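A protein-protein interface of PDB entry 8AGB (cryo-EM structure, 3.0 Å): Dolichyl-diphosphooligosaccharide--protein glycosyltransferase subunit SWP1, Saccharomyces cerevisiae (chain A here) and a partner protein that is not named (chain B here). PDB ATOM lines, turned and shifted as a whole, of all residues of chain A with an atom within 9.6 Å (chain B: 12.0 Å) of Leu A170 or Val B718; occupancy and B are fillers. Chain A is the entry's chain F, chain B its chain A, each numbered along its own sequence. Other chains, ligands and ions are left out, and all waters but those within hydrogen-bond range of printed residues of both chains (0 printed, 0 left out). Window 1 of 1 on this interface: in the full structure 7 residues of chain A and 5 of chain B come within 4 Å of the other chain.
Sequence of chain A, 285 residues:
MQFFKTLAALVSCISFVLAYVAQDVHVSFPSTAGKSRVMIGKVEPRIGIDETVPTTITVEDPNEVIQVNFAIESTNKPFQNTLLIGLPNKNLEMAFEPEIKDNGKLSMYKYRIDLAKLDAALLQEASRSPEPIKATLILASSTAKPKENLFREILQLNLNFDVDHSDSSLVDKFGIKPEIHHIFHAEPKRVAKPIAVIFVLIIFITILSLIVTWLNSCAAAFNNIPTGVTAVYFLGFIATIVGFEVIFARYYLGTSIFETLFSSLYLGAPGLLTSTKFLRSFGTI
Of the 5 printed residues of chain B, 4 touch a printed residue of chain A. Hydrophobic or aromatic side chains of chain B that line the printed part of chain A: Leu B716 and Val B718. Of the 23 printed residues of chain A, 6 touch a printed residue of chain B. Hydrophobic or aromatic side chains of chain A within 4 Å of the printed part of chain B: Leu A92, Leu A170 and Val A171.
Of the printed residues of chain B, Glu A93 touches Leu B716 (3.2 Å). Printed residues of chain B within 4 Å of Asp A119: Gly B715 (3.7 Å) and Leu B716 (3.4 Å). No residue of chain B comes within 4 Å of Ala A121. Ser A168 touches none of the printed residues of chain B. Of chain B, only Val B718 comes within 4 Å of Leu A170. No residue of chain B comes within 4 Å of Asp A172. No residue of chain B comes within 4 Å of Lys A173. No residue of chain B comes within 4 Å of Phe A174. Of the printed residues of chain A, Gly B715 touches Asp A119 (3.7 Å). Of the printed residues of chain A, Arg B717 touches Asn A91 and Leu A92. Of chain A, only Leu A170 and Val A171 come within 4 Å of Val B718. The nearest residue of chain B that does not touch Leu A170 is Leu B716 (6.4 Å). The nearest residue of chain A that does not touch Val B718 is Leu A92 (4.4 Å).
Among the printed residues, pairs that only touch across the chains: Asn A91 with Arg B717, Leu A92 with Leu B716, Leu A92 with Arg B717, Glu A93 with Leu B716, Asp A119 with Gly B715, Leu A170 with Val B718 and Val A171 with Val B718.
N of Leu A87 sits at hydrogen-bond distance from OE2 of Glu A93, at 2.9 Å. OD2 of Asp A119 lies close to N of Ala A121.
The side-chain carboxylate of Asp A119 is in hydrogen-bond range of the backbone NH of Leu B716, at 3.4 Å.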
ATOM      1  N   LEU A  87      16.529  17.564 -21.847  1.00  0.00           N
ATOM      2  CA  LEU A  87      16.405  16.553 -22.896  1.00  0.00           C
ATOM      3  C   LEU A  87      17.360  16.898 -24.030  1.00  0.00           C
ATOM      4  O   LEU A  87      17.036  17.750 -24.875  1.00  0.00           O
ATOM      5  CB  LEU A  87      14.978  16.448 -23.423  1.00  0.00           C
ATOM      6  CG  LEU A  87      13.790  16.476 -22.462  1.00  0.00           C
ATOM      7  CD1 LEU A  87      13.370  17.901 -22.153  1.00  0.00           C
ATOM      8  CD2 LEU A  87      12.627  15.692 -23.040  1.00  0.00           C
ATOM      9  N   ASN A  89      18.087  15.505 -26.750  1.00  0.00           N
ATOM     10  CA  ASN A  89      17.556  15.278 -28.087  1.00  0.00           C
ATOM     11  C   ASN A  89      16.759  16.470 -28.598  1.00  0.00           C
ATOM     12  O   ASN A  89      16.542  16.584 -29.809  1.00  0.00           O
ATOM     13  CB  ASN A  89      16.682  14.022 -28.103  1.00  0.00           C
ATOM     14  CG  ASN A  89      17.445  12.775 -27.701  1.00  0.00           C
ATOM     15  OD1 ASN A  89      17.815  11.961 -28.547  1.00  0.00           O
ATOM     16  ND2 ASN A  89      17.678  12.615 -26.403  1.00  0.00           N
ATOM     17  N   LYS A  90      16.316  17.359 -27.706  1.00  0.00           N
ATOM     18  CA  LYS A  90      15.554  18.537 -28.093  1.00  0.00           C
ATOM     19  C   LYS A  90      16.250  19.851 -27.767  1.00  0.00           C
ATOM     20  O   LYS A  90      15.677  20.913 -28.033  1.00  0.00           O
ATOM     21  CB  LYS A  90      14.172  18.514 -27.429  1.00  0.00           C
ATOM     22  CG  LYS A  90      13.135  17.745 -28.221  1.00  0.00           C
ATOM     23  CD  LYS A  90      11.860  17.548 -27.426  1.00  0.00           C
ATOM     24  CE  LYS A  90      10.757  16.989 -28.306  1.00  0.00           C
ATOM     25  NZ  LYS A  90      11.307  16.141 -29.400  1.00  0.00           N
ATOM     26  N   ASN A  91      17.451  19.812 -27.185  1.00  0.00           N
ATOM     27  CA  ASN A  91      18.241  21.013 -26.905  1.00  0.00           C
ATOM     28  C   ASN A  91      17.524  21.940 -25.923  1.00  0.00           C
ATOM     29  O   ASN A  91      17.372  23.140 -26.162  1.00  0.00           O
ATOM     30  CB  ASN A  91      18.590  21.749 -28.202  1.00  0.00           C
ATOM     31  CG  ASN A  91      18.987  20.805 -29.319  1.00  0.00           C
ATOM     32  OD1 ASN A  91      19.769  19.878 -29.117  1.00  0.00           O
ATOM     33  ND2 ASN A  91      18.441  21.033 -30.506  1.00  0.00           N
ATOM     34  N   LEU A  92      17.080  21.373 -24.801  1.00  0.00           N
ATOM     35  CA  LEU A  92      16.363  22.120 -23.774  1.00  0.00           C
ATOM     36  C   LEU A  92      17.024  21.993 -22.404  1.00  0.00           C
ATOM     37  O   LEU A  92      16.350  22.056 -21.375  1.00  0.00           O
ATOM     38  CB  LEU A  92      14.904  21.670 -23.702  1.00  0.00           C
ATOM     39  CG  LEU A  92      13.882  22.611 -24.341  1.00  0.00           C
ATOM     40  CD1 LEU A  92      12.481  22.051 -24.194  1.00  0.00           C
ATOM     41  CD2 LEU A  92      13.973  23.992 -23.721  1.00  0.00           C
ATOM     42  N   GLU A  93      18.342  21.812 -22.374  1.00  0.00           N
ATOM     43  CA  GLU A  93      19.052  21.676 -21.113  1.00  0.00           C
ATOM     44  C   GLU A  93      19.026  22.973 -20.311  1.00  0.00           C
ATOM     45  O   GLU A  93      18.724  24.054 -20.821  1.00  0.00           O
ATOM     46  CB  GLU A  93      20.500  21.259 -21.356  1.00  0.00           C
ATOM     47  CG  GLU A  93      20.740  19.782 -21.178  1.00  0.00           C
ATOM     48  CD  GLU A  93      20.016  18.960 -22.214  1.00  0.00           C
ATOM     49  OE1 GLU A  93      20.044  19.337 -23.404  1.00  0.00           O
ATOM     50  OE2 GLU A  93      19.401  17.946 -21.830  1.00  0.00           O
ATOM     51  N   ASP A 119      12.331  25.797 -15.780  1.00  0.00           N
ATOM     52  CA  ASP A 119      11.834  26.595 -16.892  1.00  0.00           C
ATOM     53  C   ASP A 119      10.481  26.061 -17.342  1.00  0.00           C
ATOM     54  O   ASP A 119      10.257  24.848 -17.373  1.00  0.00           O
ATOM     55  CB  ASP A 119      12.828  26.573 -18.053  1.00  0.00           C
ATOM     56  CG  ASP A 119      12.637  27.732 -19.005  1.00  0.00           C
ATOM     57  OD1 ASP A 119      13.039  28.860 -18.654  1.00  0.00           O
ATOM     58  OD2 ASP A 119      12.087  27.514 -20.104  1.00  0.00           O
ATOM     59  N   ALA A 120       9.566  26.976 -17.672  1.00  0.00           N
ATOM     60  CA  ALA A 120       8.242  26.566 -18.128  1.00  0.00           C
ATOM     61  C   ALA A 120       8.329  25.611 -19.311  1.00  0.00           C
ATOM     62  O   ALA A 120       7.700  24.547 -19.314  1.00  0.00           O
ATOM     63  CB  ALA A 120       7.411  27.797 -18.488  1.00  0.00           C
ATOM     64  N   ALA A 121       9.098  25.985 -20.337  1.00  0.00           N
ATOM     65  CA  ALA A 121       9.199  25.154 -21.532  1.00  0.00           C
ATOM     66  C   ALA A 121       9.735  23.760 -21.232  1.00  0.00           C
ATOM     67  O   ALA A 121       9.403  22.811 -21.956  1.00  0.00           O
ATOM     68  CB  ALA A 121      10.087  25.837 -22.572  1.00  0.00           C
ATOM     69  N   LEU A 122      10.432  23.586 -20.107  1.00  0.00           N
ATOM     70  CA  LEU A 122      10.979  22.274 -19.797  1.00  0.00           C
ATOM     71  C   LEU A 122       9.931  21.381 -19.153  1.00  0.00           C
ATOM     72  O   LEU A 122       9.800  20.213 -19.531  1.00  0.00           O
ATOM     73  CB  LEU A 122      12.192  22.433 -18.877  1.00  0.00           C
ATOM     74  CG  LEU A 122      12.948  21.207 -18.357  1.00  0.00           C
ATOM     75  CD1 LEU A 122      13.001  20.102 -19.396  1.00  0.00           C
ATOM     76  CD2 LEU A 122      14.350  21.594 -17.916  1.00  0.00           C
ATOM     77  N   GLN A 124       6.691  21.650 -19.456  1.00  0.00           N
ATOM     78  CA  GLN A 124       5.682  21.397 -20.473  1.00  0.00           C
ATOM     79  C   GLN A 124       6.193  20.434 -21.539  1.00  0.00           C
ATOM     80  O   GLN A 124       5.433  19.593 -22.030  1.00  0.00           O
ATOM     81  CB  GLN A 124       5.216  22.725 -21.067  1.00  0.00           C
ATOM     82  CG  GLN A 124       4.508  23.583 -20.025  1.00  0.00           C
ATOM     83  CD  GLN A 124       4.634  25.066 -20.279  1.00  0.00           C
ATOM     84  OE1 GLN A 124       4.298  25.885 -19.423  1.00  0.00           O
ATOM     85  NE2 GLN A 124       5.139  25.423 -21.445  1.00  0.00           N
ATOM     86  N   GLU A 125       7.477  20.529 -21.911  1.00  0.00           N
ATOM     87  CA  GLU A 125       7.993  19.581 -22.893  1.00  0.00           C
ATOM     88  C   GLU A 125       8.138  18.188 -22.291  1.00  0.00           C
ATOM     89  O   GLU A 125       7.886  17.184 -22.974  1.00  0.00           O
ATOM     90  CB  GLU A 125       9.333  20.068 -23.444  1.00  0.00           C
ATOM     91  CG  GLU A 125       9.921  19.273 -24.622  1.00  0.00           C
ATOM     92  CD  GLU A 125       8.946  19.010 -25.769  1.00  0.00           C
ATOM     93  OE1 GLU A 125       7.912  18.335 -25.573  1.00  0.00           O
ATOM     94  OE2 GLU A 125       9.219  19.494 -26.888  1.00  0.00           O
ATOM     95  N   ARG A 128       4.274  16.962 -22.329  1.00  0.00           N
ATOM     96  CA  ARG A 128       3.812  16.667 -23.681  1.00  0.00           C
ATOM     97  C   ARG A 128       4.485  15.417 -24.234  1.00  0.00           C
ATOM     98  O   ARG A 128       3.821  14.536 -24.792  1.00  0.00           O
ATOM     99  CB  ARG A 128       4.068  17.862 -24.602  1.00  0.00           C
ATOM    100  CG  ARG A 128       2.937  18.874 -24.645  1.00  0.00           C
ATOM    101  CD  ARG A 128       3.422  20.215 -25.170  1.00  0.00           C
ATOM    102  NE  ARG A 128       4.583  20.067 -26.044  1.00  0.00           N
ATOM    103  CZ  ARG A 128       4.521  20.028 -27.371  1.00  0.00           C
ATOM    104  NH1 ARG A 128       5.630  19.890 -28.084  1.00  0.00           N
ATOM    105  NH2 ARG A 128       3.350  20.122 -27.986  1.00  0.00           N
ATOM    106  N   HIS A 165      -1.529  23.300 -20.675  1.00  0.00           N
ATOM    107  CA  HIS A 165      -1.077  24.040 -21.847  1.00  0.00           C
ATOM    108  C   HIS A 165      -2.044  25.135 -22.275  1.00  0.00           C
ATOM    109  O   HIS A 165      -1.931  25.638 -23.398  1.00  0.00           O
ATOM    110  CB  HIS A 165      -0.830  23.079 -23.012  1.00  0.00           C
ATOM    111  CG  HIS A 165      -0.151  21.806 -22.612  1.00  0.00           C
ATOM    112  ND1 HIS A 165       1.174  21.756 -22.239  1.00  0.00           N
ATOM    113  CD2 HIS A 165      -0.615  20.537 -22.522  1.00  0.00           C
ATOM    114  CE1 HIS A 165       1.498  20.509 -21.940  1.00  0.00           C
ATOM    115  NE2 HIS A 165       0.430  19.751 -22.103  1.00  0.00           N
ATOM    116  N   ASP A 167      -1.990  28.048 -21.401  1.00  0.00           N
ATOM    117  CA  ASP A 167      -1.039  29.101 -21.745  1.00  0.00           C
ATOM    118  C   ASP A 167       0.144  28.338 -22.331  1.00  0.00           C
ATOM    119  O   ASP A 167       1.036  27.891 -21.608  1.00  0.00           O
ATOM    120  CB  ASP A 167      -0.650  29.940 -20.533  1.00  0.00           C
ATOM    121  N   SER A 168       0.143  28.188 -23.653  1.00  0.00           N
ATOM    122  CA  SER A 168       1.070  27.269 -24.291  1.00  0.00           C
ATOM    123  C   SER A 168       2.502  27.796 -24.270  1.00  0.00           C
ATOM    124  O   SER A 168       2.768  28.976 -24.027  1.00  0.00           O
ATOM    125  CB  SER A 168       0.643  26.999 -25.734  1.00  0.00           C
ATOM    126  N   SER A 169       3.428  26.879 -24.530  1.00  0.00           N
ATOM    127  CA  SER A 169       4.852  27.151 -24.583  1.00  0.00           C
ATOM    128  C   SER A 169       5.214  27.819 -25.903  1.00  0.00           C
ATOM    129  O   SER A 169       4.475  27.744 -26.888  1.00  0.00           O
ATOM    130  CB  SER A 169       5.658  25.861 -24.437  1.00  0.00           C
ATOM    131  N   LEU A 170       6.368  28.486 -25.915  1.00  0.00           N
ATOM    132  CA  LEU A 170       6.856  29.003 -27.184  1.00  0.00           C
ATOM    133  C   LEU A 170       7.211  27.861 -28.126  1.00  0.00           C
ATOM    134  O   LEU A 170       7.343  28.081 -29.334  1.00  0.00           O
ATOM    135  CB  LEU A 170       8.061  29.918 -26.962  1.00  0.00           C
ATOM    136  N   VAL A 171       7.357  26.649 -27.590  1.00  0.00           N
ATOM    137  CA  VAL A 171       7.674  25.462 -28.372  1.00  0.00           C
ATOM    138  C   VAL A 171       6.360  24.912 -28.896  1.00  0.00           C
ATOM    139  O   VAL A 171       5.385  24.801 -28.143  1.00  0.00           O
ATOM    140  CB  VAL A 171       8.415  24.416 -27.524  1.00  0.00           C
ATOM    141  N   ASP A 172       6.318  24.602 -30.190  1.00  0.00           N
ATOM    142  CA  ASP A 172       5.176  24.039 -30.901  1.00  0.00           C
ATOM    143  C   ASP A 172       4.176  25.153 -31.185  1.00  0.00           C
ATOM    144  O   ASP A 172       3.120  24.883 -31.773  1.00  0.00           O
ATOM    145  CB  ASP A 172       4.480  22.882 -30.166  1.00  0.00           C
ATOM    146  N   LYS A 173       4.468  26.393 -30.779  1.00  0.00           N
ATOM    147  CA  LYS A 173       3.603  27.513 -31.132  1.00  0.00           C
ATOM    148  C   LYS A 173       3.593  27.716 -32.638  1.00  0.00           C
ATOM    149  O   LYS A 173       2.565  28.096 -33.210  1.00  0.00           O
ATOM    150  CB  LYS A 173       4.066  28.779 -30.412  1.00  0.00           C
ATOM    151  CG  LYS A 173       2.958  29.768 -30.102  1.00  0.00           C
ATOM    152  CD  LYS A 173       3.476  30.904 -29.234  1.00  0.00           C
ATOM    153  CE  LYS A 173       2.381  31.907 -28.915  1.00  0.00           C
ATOM    154  NZ  LYS A 173       1.823  32.536 -30.142  1.00  0.00           N
ATOM    155  N   PHE A 174       4.725  27.472 -33.288  1.00  0.00           N
ATOM    156  CA  PHE A 174       4.824  27.499 -34.738  1.00  0.00           C
ATOM    157  C   PHE A 174       4.964  26.048 -35.173  1.00  0.00           C
ATOM    158  O   PHE A 174       5.863  25.342 -34.704  1.00  0.00           O
ATOM    159  CB  PHE A 174       6.020  28.333 -35.210  1.00  0.00           C
ATOM    160  CG  PHE A 174       6.622  29.206 -34.139  1.00  0.00           C
ATOM    161  CD1 PHE A 174       5.913  30.276 -33.610  1.00  0.00           C
ATOM    162  CD2 PHE A 174       7.900  28.958 -33.665  1.00  0.00           C
ATOM    163  CE1 PHE A 174       6.467  31.075 -32.626  1.00  0.00           C
ATOM    164  CE2 PHE A 174       8.460  29.756 -32.683  1.00  0.00           C
ATOM    165  CZ  PHE A 174       7.742  30.815 -32.163  1.00  0.00           C
ATOM    166  N   GLY A 175       4.085  25.603 -36.058  1.00  0.00           N
ATOM    167  CA  GLY A 175       4.160  24.245 -36.549  1.00  0.00           C
ATOM    168  C   GLY A 175       2.793  23.783 -37.016  1.00  0.00           C
ATOM    169  O   GLY A 175       1.842  24.560 -37.080  1.00  0.00           O
ATOM    170  N   LEU B 714      17.125  35.771 -19.693  1.00  0.00           N
ATOM    171  CA  LEU B 714      15.988  35.258 -20.445  1.00  0.00           C
ATOM    172  C   LEU B 714      15.703  33.821 -20.016  1.00  0.00           C
ATOM    173  O   LEU B 714      16.305  33.295 -19.076  1.00  0.00           O
ATOM    174  CB  LEU B 714      16.265  35.352 -21.942  1.00  0.00           C
ATOM    175  CG  LEU B 714      16.798  36.684 -22.464  1.00  0.00           C
ATOM    176  CD1 LEU B 714      17.457  36.489 -23.811  1.00  0.00           C
ATOM    177  CD2 LEU B 714      15.680  37.705 -22.562  1.00  0.00           C
ATOM    178  N   GLY B 715      14.771  33.162 -20.705  1.00  0.00           N
ATOM    179  CA  GLY B 715      14.478  31.768 -20.477  1.00  0.00           C
ATOM    180  C   GLY B 715      15.029  30.897 -21.597  1.00  0.00           C
ATOM    181  O   GLY B 715      15.608  31.373 -22.570  1.00  0.00           O
ATOM    182  N   LEU B 716      14.838  29.591 -21.431  1.00  0.00           N
ATOM    183  CA  LEU B 716      15.410  28.645 -22.379  1.00  0.00           C
ATOM    184  C   LEU B 716      14.790  28.815 -23.759  1.00  0.00           C
ATOM    185  O   LEU B 716      13.565  28.866 -23.901  1.00  0.00           O
ATOM    186  CB  LEU B 716      15.184  27.218 -21.884  1.00  0.00           C
ATOM    187  CG  LEU B 716      16.365  26.458 -21.288  1.00  0.00           C
ATOM    188  CD1 LEU B 716      17.240  27.382 -20.462  1.00  0.00           C
ATOM    189  CD2 LEU B 716      15.846  25.309 -20.443  1.00  0.00           C
ATOM    190  N   ARG B 717      15.641  28.909 -24.776  1.00  0.00           N
ATOM    191  CA  ARG B 717      15.163  28.937 -26.151  1.00  0.00           C
ATOM    192  C   ARG B 717      14.611  27.564 -26.507  1.00  0.00           C
ATOM    193  O   ARG B 717      15.337  26.567 -26.426  1.00  0.00           O
ATOM    194  CB  ARG B 717      16.287  29.339 -27.100  1.00  0.00           C
ATOM    195  CG  ARG B 717      15.995  29.051 -28.556  1.00  0.00           C
ATOM    196  CD  ARG B 717      15.346  30.252 -29.210  1.00  0.00           C
ATOM    197  NE  ARG B 717      14.659  29.906 -30.448  1.00  0.00           N
ATOM    198  CZ  ARG B 717      13.985  30.775 -31.190  1.00  0.00           C
ATOM    199  NH1 ARG B 717      13.914  32.045 -30.821  1.00  0.00           N
ATOM    200  NH2 ARG B 717      13.387  30.380 -32.303  1.00  0.00           N
ATOM    201  N   VAL B 718      13.331  27.501 -26.858  1.00  0.00           N
ATOM    202  CA  VAL B 718      12.692  26.253 -27.281  1.00  0.00           C
ATOM    203  C   VAL B 718      13.566  25.420 -28.216  1.00  0.00           C
ATOM    204  O   VAL B 718      13.103  24.449 -28.814  1.00  0.00           O
ATOM    205  CB  VAL B 718      11.338  26.531 -27.927  1.00  0.00           C
ATOM    206  CG1 VAL B 718      10.481  27.327 -26.974  1.00  0.00           C
ATOM    207  CG2 VAL B 718      11.520  27.275 -29.239  1.00  0.00           C
